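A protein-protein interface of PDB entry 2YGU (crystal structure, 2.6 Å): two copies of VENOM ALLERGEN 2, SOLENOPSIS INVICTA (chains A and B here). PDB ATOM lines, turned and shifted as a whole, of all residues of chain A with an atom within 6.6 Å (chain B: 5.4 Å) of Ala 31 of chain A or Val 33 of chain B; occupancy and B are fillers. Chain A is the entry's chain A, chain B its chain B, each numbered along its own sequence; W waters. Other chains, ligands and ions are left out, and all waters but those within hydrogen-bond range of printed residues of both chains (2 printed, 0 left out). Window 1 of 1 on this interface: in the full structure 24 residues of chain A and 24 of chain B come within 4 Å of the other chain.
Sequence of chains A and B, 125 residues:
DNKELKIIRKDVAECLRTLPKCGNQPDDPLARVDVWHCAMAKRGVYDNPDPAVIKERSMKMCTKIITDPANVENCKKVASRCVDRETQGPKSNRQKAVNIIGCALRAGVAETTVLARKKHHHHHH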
ATOM      1  N   ASN A  24      -3.062  11.805  37.021  1.00  0.00           N
ATOM      2  CA  ASN A  24      -3.905  12.457  36.013  1.00  0.00           C
ATOM      3  C   ASN A  24      -4.331  11.509  34.899  1.00  0.00           C
ATOM      4  O   ASN A  24      -3.950  11.663  33.736  1.00  0.00           O
ATOM      5  CB  ASN A  24      -3.223  13.717  35.470  1.00  0.00           C
ATOM      6  CG  ASN A  24      -3.250  14.883  36.475  1.00  0.00           C
ATOM      7  OD1 ASN A  24      -4.308  15.247  37.005  1.00  0.00           O
ATOM      8  ND2 ASN A  24      -2.082  15.478  36.721  1.00  0.00           N
ATOM      9  N   GLN A  25      -5.113  10.505  35.281  1.00  0.00           N
ATOM     10  CA  GLN A  25      -5.655   9.548  34.322  1.00  0.00           C
ATOM     11  C   GLN A  25      -7.165   9.455  34.469  1.00  0.00           C
ATOM     12  O   GLN A  25      -7.681   9.471  35.585  1.00  0.00           O
ATOM     13  CB  GLN A  25      -5.005   8.165  34.491  1.00  0.00           C
ATOM     14  N   PRO A  26      -7.880   9.356  33.337  1.00  0.00           N
ATOM     15  CA  PRO A  26      -9.323   9.245  33.400  1.00  0.00           C
ATOM     16  C   PRO A  26      -9.750   7.936  34.018  1.00  0.00           C
ATOM     17  O   PRO A  26      -9.063   6.934  33.853  1.00  0.00           O
ATOM     18  CB  PRO A  26      -9.748   9.273  31.936  1.00  0.00           C
ATOM     19  CG  PRO A  26      -8.552   9.547  31.155  1.00  0.00           C
ATOM     20  CD  PRO A  26      -7.382   9.230  31.964  1.00  0.00           C
ATOM     21  N   ASP A  27     -10.878   7.946  34.712  1.00  0.00           N
ATOM     22  CA  ASP A  27     -11.437   6.721  35.295  1.00  0.00           C
ATOM     23  C   ASP A  27     -11.900   5.755  34.213  1.00  0.00           C
ATOM     24  O   ASP A  27     -11.893   4.545  34.403  1.00  0.00           O
ATOM     25  CB  ASP A  27     -12.605   7.044  36.221  1.00  0.00           C
ATOM     26  CG  ASP A  27     -12.166   7.738  37.489  1.00  0.00           C
ATOM     27  OD1 ASP A  27     -10.989   7.567  37.876  1.00  0.00           O
ATOM     28  OD2 ASP A  27     -12.991   8.446  38.106  1.00  0.00           O
ATOM     29  N   ASP A  28     -12.292   6.303  33.073  1.00  0.00           N
ATOM     30  CA  ASP A  28     -12.757   5.494  31.945  1.00  0.00           C
ATOM     31  C   ASP A  28     -11.592   4.804  31.215  1.00  0.00           C
ATOM     32  O   ASP A  28     -10.801   5.467  30.550  1.00  0.00           O
ATOM     33  CB  ASP A  28     -13.552   6.371  30.972  1.00  0.00           C
ATOM     34  CG  ASP A  28     -13.973   5.633  29.710  1.00  0.00           C
ATOM     35  OD1 ASP A  28     -14.019   4.381  29.719  1.00  0.00           O
ATOM     36  OD2 ASP A  28     -14.256   6.323  28.700  1.00  0.00           O
ATOM     37  N   PRO A  29     -11.499   3.465  31.319  1.00  0.00           N
ATOM     38  CA  PRO A  29     -10.362   2.771  30.728  1.00  0.00           C
ATOM     39  C   PRO A  29     -10.279   2.917  29.222  1.00  0.00           C
ATOM     40  O   PRO A  29      -9.181   2.910  28.657  1.00  0.00           O
ATOM     41  CB  PRO A  29     -10.608   1.308  31.094  1.00  0.00           C
ATOM     42  CG  PRO A  29     -12.034   1.209  31.439  1.00  0.00           C
ATOM     43  CD  PRO A  29     -12.426   2.529  31.987  1.00  0.00           C
ATOM     44  N   LEU A  30     -11.430   3.057  28.572  1.00  0.00           N
ATOM     45  CA  LEU A  30     -11.468   3.187  27.110  1.00  0.00           C
ATOM     46  C   LEU A  30     -11.027   4.587  26.659  1.00  0.00           C
ATOM     47  O   LEU A  30     -10.894   4.850  25.461  1.00  0.00           O
ATOM     48  CB  LEU A  30     -12.863   2.859  26.574  1.00  0.00           C
ATOM     49  CG  LEU A  30     -13.368   1.446  26.906  1.00  0.00           C
ATOM     50  CD1 LEU A  30     -14.787   1.251  26.423  1.00  0.00           C
ATOM     51  CD2 LEU A  30     -12.448   0.384  26.298  1.00  0.00           C
ATOM     52  N   ALA A  31     -10.812   5.484  27.617  1.00  0.00           N
ATOM     53  CA  ALA A  31     -10.250   6.807  27.336  1.00  0.00           C
ATOM     54  C   ALA A  31      -8.730   6.824  27.527  1.00  0.00           C
ATOM     55  O   ALA A  31      -8.100   7.872  27.384  1.00  0.00           O
ATOM     56  CB  ALA A  31     -10.902   7.863  28.233  1.00  0.00           C
ATOM     57  N   ARG A  32      -8.145   5.668  27.848  1.00  0.00           N
ATOM     58  CA  ARG A  32      -6.714   5.586  28.164  1.00  0.00           C
ATOM     59  C   ARG A  32      -5.893   4.900  27.083  1.00  0.00           C
ATOM     60  O   ARG A  32      -6.180   3.781  26.691  1.00  0.00           O
ATOM     61  CB  ARG A  32      -6.509   4.840  29.469  1.00  0.00           C
ATOM     62  CG  ARG A  32      -6.842   5.662  30.673  1.00  0.00           C
ATOM     63  CD  ARG A  32      -6.793   4.860  31.951  1.00  0.00           C
ATOM     64  NE  ARG A  32      -5.485   4.267  32.171  1.00  0.00           N
ATOM     65  CZ  ARG A  32      -5.142   3.604  33.264  1.00  0.00           C
ATOM     66  NH1 ARG A  32      -6.004   3.445  34.261  1.00  0.00           N
ATOM     67  NH2 ARG A  32      -3.922   3.094  33.353  1.00  0.00           N
ATOM     68  N   VAL A  33      -4.836   5.576  26.646  1.00  0.00           N
ATOM     69  CA  VAL A  33      -3.952   5.033  25.613  1.00  0.00           C
ATOM     70  C   VAL A  33      -3.266   3.753  26.084  1.00  0.00           C
ATOM     71  O   VAL A  33      -3.193   2.784  25.356  1.00  0.00           O
ATOM     72  CB  VAL A  33      -2.850   6.026  25.200  1.00  0.00           C
ATOM     73  CG1 VAL A  33      -1.840   5.348  24.302  1.00  0.00           C
ATOM     74  CG2 VAL A  33      -3.452   7.236  24.498  1.00  0.00           C
ATOM     75  N   VAL A  35      -4.176   1.548  28.251  1.00  0.00           N
ATOM     76  CA  VAL A  35      -5.121   0.430  28.306  1.00  0.00           C
ATOM     77  C   VAL A  35      -5.406  -0.129  26.925  1.00  0.00           C
ATOM     78  O   VAL A  35      -5.365  -1.342  26.716  1.00  0.00           O
ATOM     79  CB  VAL A  35      -6.445   0.823  28.955  1.00  0.00           C
ATOM     80  CG1 VAL A  35      -7.480  -0.303  28.789  1.00  0.00           C
ATOM     81  CG2 VAL A  35      -6.220   1.152  30.437  1.00  0.00           C
ATOM     82  N   TRP A  36      -5.706   0.751  25.976  1.00  0.00           N
ATOM     83  CA  TRP A  36      -5.978   0.312  24.604  1.00  0.00           C
ATOM     84  C   TRP A  36      -4.786  -0.424  24.025  1.00  0.00           C
ATOM     85  O   TRP A  36      -4.934  -1.503  23.471  1.00  0.00           O
ATOM     86  CB  TRP A  36      -6.309   1.492  23.715  1.00  0.00           C
ATOM     87  CG  TRP A  36      -7.744   1.829  23.712  1.00  0.00           C
ATOM     88  CD1 TRP A  36      -8.332   2.882  24.315  1.00  0.00           C
ATOM     89  CD2 TRP A  36      -8.784   1.112  23.054  1.00  0.00           C
ATOM     90  NE1 TRP A  36      -9.680   2.867  24.089  1.00  0.00           N
ATOM     91  CE2 TRP A  36      -9.984   1.789  23.315  1.00  0.00           C
ATOM     92  CE3 TRP A  36      -8.820  -0.047  22.279  1.00  0.00           C
ATOM     93  CZ2 TRP A  36     -11.204   1.355  22.827  1.00  0.00           C
ATOM     94  CZ3 TRP A  36     -10.035  -0.471  21.786  1.00  0.00           C
ATOM     95  CH2 TRP A  36     -11.209   0.224  22.063  1.00  0.00           C
ATOM     96  N   LEU A 105      -6.889   7.034  18.992  1.00  0.00           N
ATOM     97  CA  LEU A 105      -7.726   7.543  20.085  1.00  0.00           C
ATOM     98  C   LEU A 105      -8.074   8.996  19.826  1.00  0.00           C
ATOM     99  O   LEU A 105      -9.215   9.405  19.916  1.00  0.00           O
ATOM    100  CB  LEU A 105      -7.012   7.427  21.420  1.00  0.00           C
ATOM    101  CG  LEU A 105      -7.904   7.743  22.630  1.00  0.00           C
ATOM    102  CD1 LEU A 105      -8.796   6.565  22.946  1.00  0.00           C
ATOM    103  CD2 LEU A 105      -7.083   8.114  23.863  1.00  0.00           C
ATOM    104  N   ALA A 110     -12.222   5.214  19.284  1.00  0.00           N
ATOM    105  CA  ALA A 110     -12.647   4.505  20.503  1.00  0.00           C
ATOM    106  C   ALA A 110     -14.132   4.692  20.766  1.00  0.00           C
ATOM    107  O   ALA A 110     -14.820   3.767  21.209  1.00  0.00           O
ATOM    108  CB  ALA A 110     -11.845   4.938  21.695  1.00  0.00           C
ATOM    109  N   ALA B  31      -2.461  13.952  22.227  1.00  0.00           N
ATOM    110  CA  ALA B  31      -3.078  12.639  22.437  1.00  0.00           C
ATOM    111  C   ALA B  31      -3.142  12.279  23.917  1.00  0.00           C
ATOM    112  O   ALA B  31      -3.584  11.189  24.268  1.00  0.00           O
ATOM    113  CB  ALA B  31      -2.304  11.567  21.672  1.00  0.00           C
ATOM    114  N   ARG B  32      -2.709  13.190  24.788  1.00  0.00           N
ATOM    115  CA  ARG B  32      -2.613  12.904  26.229  1.00  0.00           C
ATOM    116  C   ARG B  32      -3.655  13.635  27.047  1.00  0.00           C
ATOM    117  O   ARG B  32      -3.780  14.854  26.965  1.00  0.00           O
ATOM    118  CB  ARG B  32      -1.243  13.287  26.749  1.00  0.00           C
ATOM    119  CG  ARG B  32      -0.178  12.302  26.367  1.00  0.00           C
ATOM    120  CD  ARG B  32       1.205  12.782  26.744  1.00  0.00           C
ATOM    121  NE  ARG B  32       1.318  13.048  28.172  1.00  0.00           N
ATOM    122  CZ  ARG B  32       2.452  13.363  28.784  1.00  0.00           C
ATOM    123  NH1 ARG B  32       3.592  13.467  28.099  1.00  0.00           N
ATOM    124  NH2 ARG B  32       2.442  13.581  30.092  1.00  0.00           N
ATOM    125  N   VAL B  33      -4.376  12.882  27.869  1.00  0.00           N
ATOM    126  CA  VAL B  33      -5.418  13.458  28.722  1.00  0.00           C
ATOM    127  C   VAL B  33      -4.831  14.435  29.735  1.00  0.00           C
ATOM    128  O   VAL B  33      -5.367  15.519  29.942  1.00  0.00           O
ATOM    129  CB  VAL B  33      -6.196  12.379  29.510  1.00  0.00           C
ATOM    130  CG1 VAL B  33      -7.105  13.042  30.534  1.00  0.00           C
ATOM    131  CG2 VAL B  33      -7.009  11.506  28.577  1.00  0.00           C
ATOM    132  N   ASP B  34      -3.727  14.048  30.361  1.00  0.00           N
ATOM    133  CA  ASP B  34      -3.121  14.872  31.399  1.00  0.00           C
ATOM    134  C   ASP B  34      -2.643  16.226  30.843  1.00  0.00           C
ATOM    135  O   ASP B  34      -2.759  17.244  31.520  1.00  0.00           O
ATOM    136  CB  ASP B  34      -2.008  14.132  32.173  1.00  0.00           C
ATOM    137  CG  ASP B  34      -0.866  13.681  31.298  1.00  0.00           C
ATOM    138  OD1 ASP B  34      -1.075  13.532  30.073  1.00  0.00           O
ATOM    139  OD2 ASP B  34       0.251  13.464  31.843  1.00  0.00           O
ATOM    140  N   VAL B  35      -2.155  16.236  29.607  1.00  0.00           N
ATOM    141  CA  VAL B  35      -1.733  17.476  28.956  1.00  0.00           C
ATOM    142  C   VAL B  35      -2.908  18.382  28.640  1.00  0.00           C
ATOM    143  O   VAL B  35      -2.858  19.592  28.902  1.00  0.00           O
ATOM    144  CB  VAL B  35      -0.959  17.223  27.662  1.00  0.00           C
ATOM    145  CG1 VAL B  35      -0.735  18.533  26.903  1.00  0.00           C
ATOM    146  CG2 VAL B  35       0.365  16.546  27.964  1.00  0.00           C
ATOM    147  N   TRP B  36      -3.960  17.812  28.066  1.00  0.00           N
ATOM    148  CA  TRP B  36      -5.164  18.598  27.737  1.00  0.00           C
ATOM    149  C   TRP B  36      -5.777  19.184  28.995  1.00  0.00           C
ATOM    150  O   TRP B  36      -6.062  20.364  29.059  1.00  0.00           O
ATOM    151  CB  TRP B  36      -6.203  17.726  27.047  1.00  0.00           C
ATOM    152  CG  TRP B  36      -6.045  17.687  25.572  1.00  0.00           C
ATOM    153  CD1 TRP B  36      -5.556  16.666  24.831  1.00  0.00           C
ATOM    154  CD2 TRP B  36      -6.353  18.739  24.655  1.00  0.00           C
ATOM    155  NE1 TRP B  36      -5.559  16.998  23.509  1.00  0.00           N
ATOM    156  CE2 TRP B  36      -6.031  18.277  23.377  1.00  0.00           C
ATOM    157  CE3 TRP B  36      -6.863  20.021  24.795  1.00  0.00           C
ATOM    158  CZ2 TRP B  36      -6.217  19.043  22.250  1.00  0.00           C
ATOM    159  CZ3 TRP B  36      -7.056  20.778  23.675  1.00  0.00           C
ATOM    160  CH2 TRP B  36      -6.741  20.288  22.417  1.00  0.00           C
ATOM    161  N   HIS B  37      -5.953  18.346  30.009  1.00  0.00           N
ATOM    162  CA  HIS B  37      -6.517  18.801  31.273  1.00  0.00           C
ATOM    163  C   HIS B  37      -5.673  19.886  31.904  1.00  0.00           C
ATOM    164  O   HIS B  37      -6.186  20.878  32.410  1.00  0.00           O
ATOM    165  CB  HIS B  37      -6.616  17.664  32.275  1.00  0.00           C
ATOM    166  CG  HIS B  37      -6.874  18.130  33.670  1.00  0.00           C
ATOM    167  ND1 HIS B  37      -5.872  18.252  34.607  1.00  0.00           N
ATOM    168  CD2 HIS B  37      -8.012  18.558  34.270  1.00  0.00           C
ATOM    169  CE1 HIS B  37      -6.388  18.705  35.737  1.00  0.00           C
ATOM    170  NE2 HIS B  37      -7.683  18.897  35.558  1.00  0.00           N
ATOM    171  N   CYS B  38      -4.369  19.663  31.909  1.00  0.00           N
ATOM    172  CA  CYS B  38      -3.427  20.645  32.424  1.00  0.00           C
ATOM    173  C   CYS B  38      -3.584  21.973  31.676  1.00  0.00           C
ATOM    174  O   CYS B  38      -3.683  23.033  32.291  1.00  0.00           O
ATOM    175  CB  CYS B  38      -2.005  20.120  32.280  1.00  0.00           C
ATOM    176  SG  CYS B  38      -0.716  21.256  32.818  1.00  0.00           S
ATOM    177  N   VAL B  98     -10.621  15.845  34.982  1.00  0.00           N
ATOM    178  CA  VAL B  98      -9.828  14.899  34.187  1.00  0.00           C
ATOM    179  C   VAL B  98     -10.738  13.959  33.406  1.00  0.00           C
ATOM    180  O   VAL B  98     -10.502  13.687  32.236  1.00  0.00           O
ATOM    181  CB  VAL B  98      -8.880  14.061  35.089  1.00  0.00           C
ATOM    182  CG1 VAL B  98      -8.269  12.916  34.315  1.00  0.00           C
ATOM    183  CG2 VAL B  98      -7.784  14.965  35.703  1.00  0.00           C
ATOM    184  N   ILE B 101     -12.276  15.657  30.344  1.00  0.00           N
ATOM    185  CA  ILE B 101     -11.273  15.737  29.285  1.00  0.00           C
ATOM    186  C   ILE B 101     -11.124  14.389  28.586  1.00  0.00           C
ATOM    187  O   ILE B 101     -11.075  14.308  27.363  1.00  0.00           O
ATOM    188  CB  ILE B 101      -9.914  16.201  29.843  1.00  0.00           C
ATOM    189  CG1 ILE B 101      -9.983  17.696  30.149  1.00  0.00           C
ATOM    190  CG2 ILE B 101      -8.785  15.938  28.859  1.00  0.00           C
ATOM    191  CD1 ILE B 101     -10.070  18.578  28.923  1.00  0.00           C
ATOM    192  N   GLY B 102     -11.073  13.331  29.368  1.00  0.00           N
ATOM    193  CA  GLY B 102     -10.966  11.988  28.812  1.00  0.00           C
ATOM    194  C   GLY B 102     -12.149  11.658  27.918  1.00  0.00           C
ATOM    195  O   GLY B 102     -12.001  11.006  26.872  1.00  0.00           O
ATOM    196  N   CYS B 103     -13.322  12.120  28.323  1.00  0.00           N
ATOM    197  CA  CYS B 103     -14.566  11.891  27.574  1.00  0.00           C
ATOM    198  C   CYS B 103     -14.543  12.627  26.229  1.00  0.00           C
ATOM    199  O   CYS B 103     -14.970  12.098  25.204  1.00  0.00           O
ATOM    200  CB  CYS B 103     -15.781  12.324  28.419  1.00  0.00           C
ATOM    201  SG  CYS B 103     -17.391  12.359  27.561  1.00  0.00           S
ATOM    202  N   LEU B 105     -11.746  13.620  24.665  1.00  0.00           N
ATOM    203  CA  LEU B 105     -10.653  13.058  23.866  1.00  0.00           C
ATOM    204  C   LEU B 105     -11.126  11.787  23.166  1.00  0.00           C
ATOM    205  O   LEU B 105     -10.917  11.582  21.967  1.00  0.00           O
ATOM    206  CB  LEU B 105      -9.446  12.727  24.739  1.00  0.00           C
ATOM    207  CG  LEU B 105      -8.190  12.327  23.941  1.00  0.00           C
ATOM    208  CD1 LEU B 105      -7.507  13.550  23.388  1.00  0.00           C
ATOM    209  CD2 LEU B 105      -7.227  11.525  24.786  1.00  0.00           C
ATOM    210  N   ARG B 106     -11.790  10.938  23.932  1.00  0.00           N
ATOM    211  CA  ARG B 106     -12.326   9.702  23.400  1.00  0.00           C
ATOM    212  C   ARG B 106     -13.287   9.962  22.250  1.00  0.00           C
ATOM    213  O   ARG B 106     -13.309   9.200  21.284  1.00  0.00           O
ATOM    214  CB  ARG B 106     -13.048   8.935  24.495  1.00  0.00           C
ATOM    215  CG  ARG B 106     -13.153   7.457  24.215  1.00  0.00           C
ATOM    216  CD  ARG B 106     -14.019   6.773  25.243  1.00  0.00           C
ATOM    217  NE  ARG B 106     -15.433   6.944  24.936  1.00  0.00           N
ATOM    218  CZ  ARG B 106     -16.429   6.436  25.649  1.00  0.00           C
ATOM    219  NH1 ARG B 106     -16.182   5.720  26.739  1.00  0.00           N
ATOM    220  NH2 ARG B 106     -17.676   6.642  25.265  1.00  0.00           N
HETATM  221  O   HOH W   1     -11.310   7.692  20.307  1.00  0.00           O
HETATM  222  O   HOH W   2      -3.369  17.388  34.202  1.00  0.00           O
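Water W2 lies within hydrogen-bond range of a ring nitrogen (ND1) of His 37 of chain B, the backbone carbonyl oxygen of Asp 34 of chain B, the backbone NH of Cys 38 of chain B and the side-chain amide nitrogen of Asn 24 of chain A.
Water W1 lies within hydrogen-bond range of the backbone carbonyl oxygen (O) of Arg 106 of chain B (2.7 Å), the backbone carbonyl oxygen (O) of Leu 105 of chain A (2.7 Å) and the backbone NH (N) of Ala 110 of chain A (2.8 Å).
OD2 of Asp 34 of chain B lies within salt-bridge range of NH2 of Arg 32 of chain B (2.8 Å).
The indole nitrogen (NE1) of Trp 36 of chain A is in hydrogen-bond range of the backbone carbonyl oxygen (O) of Leu 30 of chain A (2.7 Å).
The side-chain carboxylate (OD1) of Asp 28 of chain A is in hydrogen-bond range of the backbone NH (N) of Leu 30 of chain A, at 3.1 Å.
The side-chain carboxylate (OD2) of Asp 28 of chain A is in salt-bridge range of the guanidinium group (NH1) of Arg 106 of chain B (2.8 Å).
O of Leu 105 of chain A lies close to O of Leu 105 of chain B (3.4 Å).
Ala 31 of chain A touches Val 33 of chain B, and with the chains exchanged Val 33 of chain A touches Ala 31 of chain B.
Leu 105 of chain B touches its own counterpart, Leu 105 of chain A.
Of chain B, only Val 33 (3.98 Å) and Gly 102 (3.6 Å) come within 4 Å of Ala 31 of chain A.
Of chain A, only Pro 26 and Ala 31 come within 4 Å of Val 33 of chain B.
Of the printed residues of chain B, Val 33 of chain A touches Ala 31 (3.96 Å).
Of the printed residues of chain A, Asp 34 of chain B touches Asn 24 (3.5 Å).
Of the printed residues of chain B, Asp 28 of chain A touches Arg 106 (2.8 Å).
Of the printed residues of chain A, Leu 105 of chain B touches Leu 105 (3.4 Å).
Of the printed residues of chain A, Val 98 of chain B touches Asn 24, Gln 25 and Pro 26.
Among the printed residues, merely in contact across the chains: Asn 24 of chain A with Asp 34 of chain B (3.5 Å), Pro 26 of chain A with Val 33 of chain B (3.6 Å), Ala 31 of chain A with Gly 102 of chain B (3.6 Å), Gln 25 of chain A with Val 98 of chain B (3.6 Å), Leu 30 of chain A with Arg 106 of chain B (3.7 Å), Pro 26 of chain A with Val 98 of chain B (3.7 Å), Asn 24 of chain A with Val 98 of chain B (3.7 Å), Ala 110 of chain A with Arg 106 of chain B (3.8 Å), Val 33 of chain A with Ala 31 of chain B (3.96 Å) and Ala 31 of chain A with Val 33 of chain B (3.98 Å).
Of the 14 printed residues of chain A, 9 touch a printed residue of chain B.
Printed residues of chain A that touch a printed residue of chain B: Asn 24, Gln 25, Pro 26, Asp 28, Leu 30, Ala 31, Val 33, Leu 105 and Ala 110.
Hydrophobic or aromatic side chains of chain A within 4 Å of the printed part of chain B: Pro 26, Ala 31, Val 33, Leu 105 and Ala 110.
Along chain A the printed residues that touch a printed residue of chain B span positions 24 to 110.
Of the 14 printed residues of chain B, 7 touch a printed residue of chain A.
Printed residues of chain B that touch a printed residue of chain A: Ala 31, Val 33, Asp 34, Val 98, Gly 102, Leu 105 and Arg 106.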
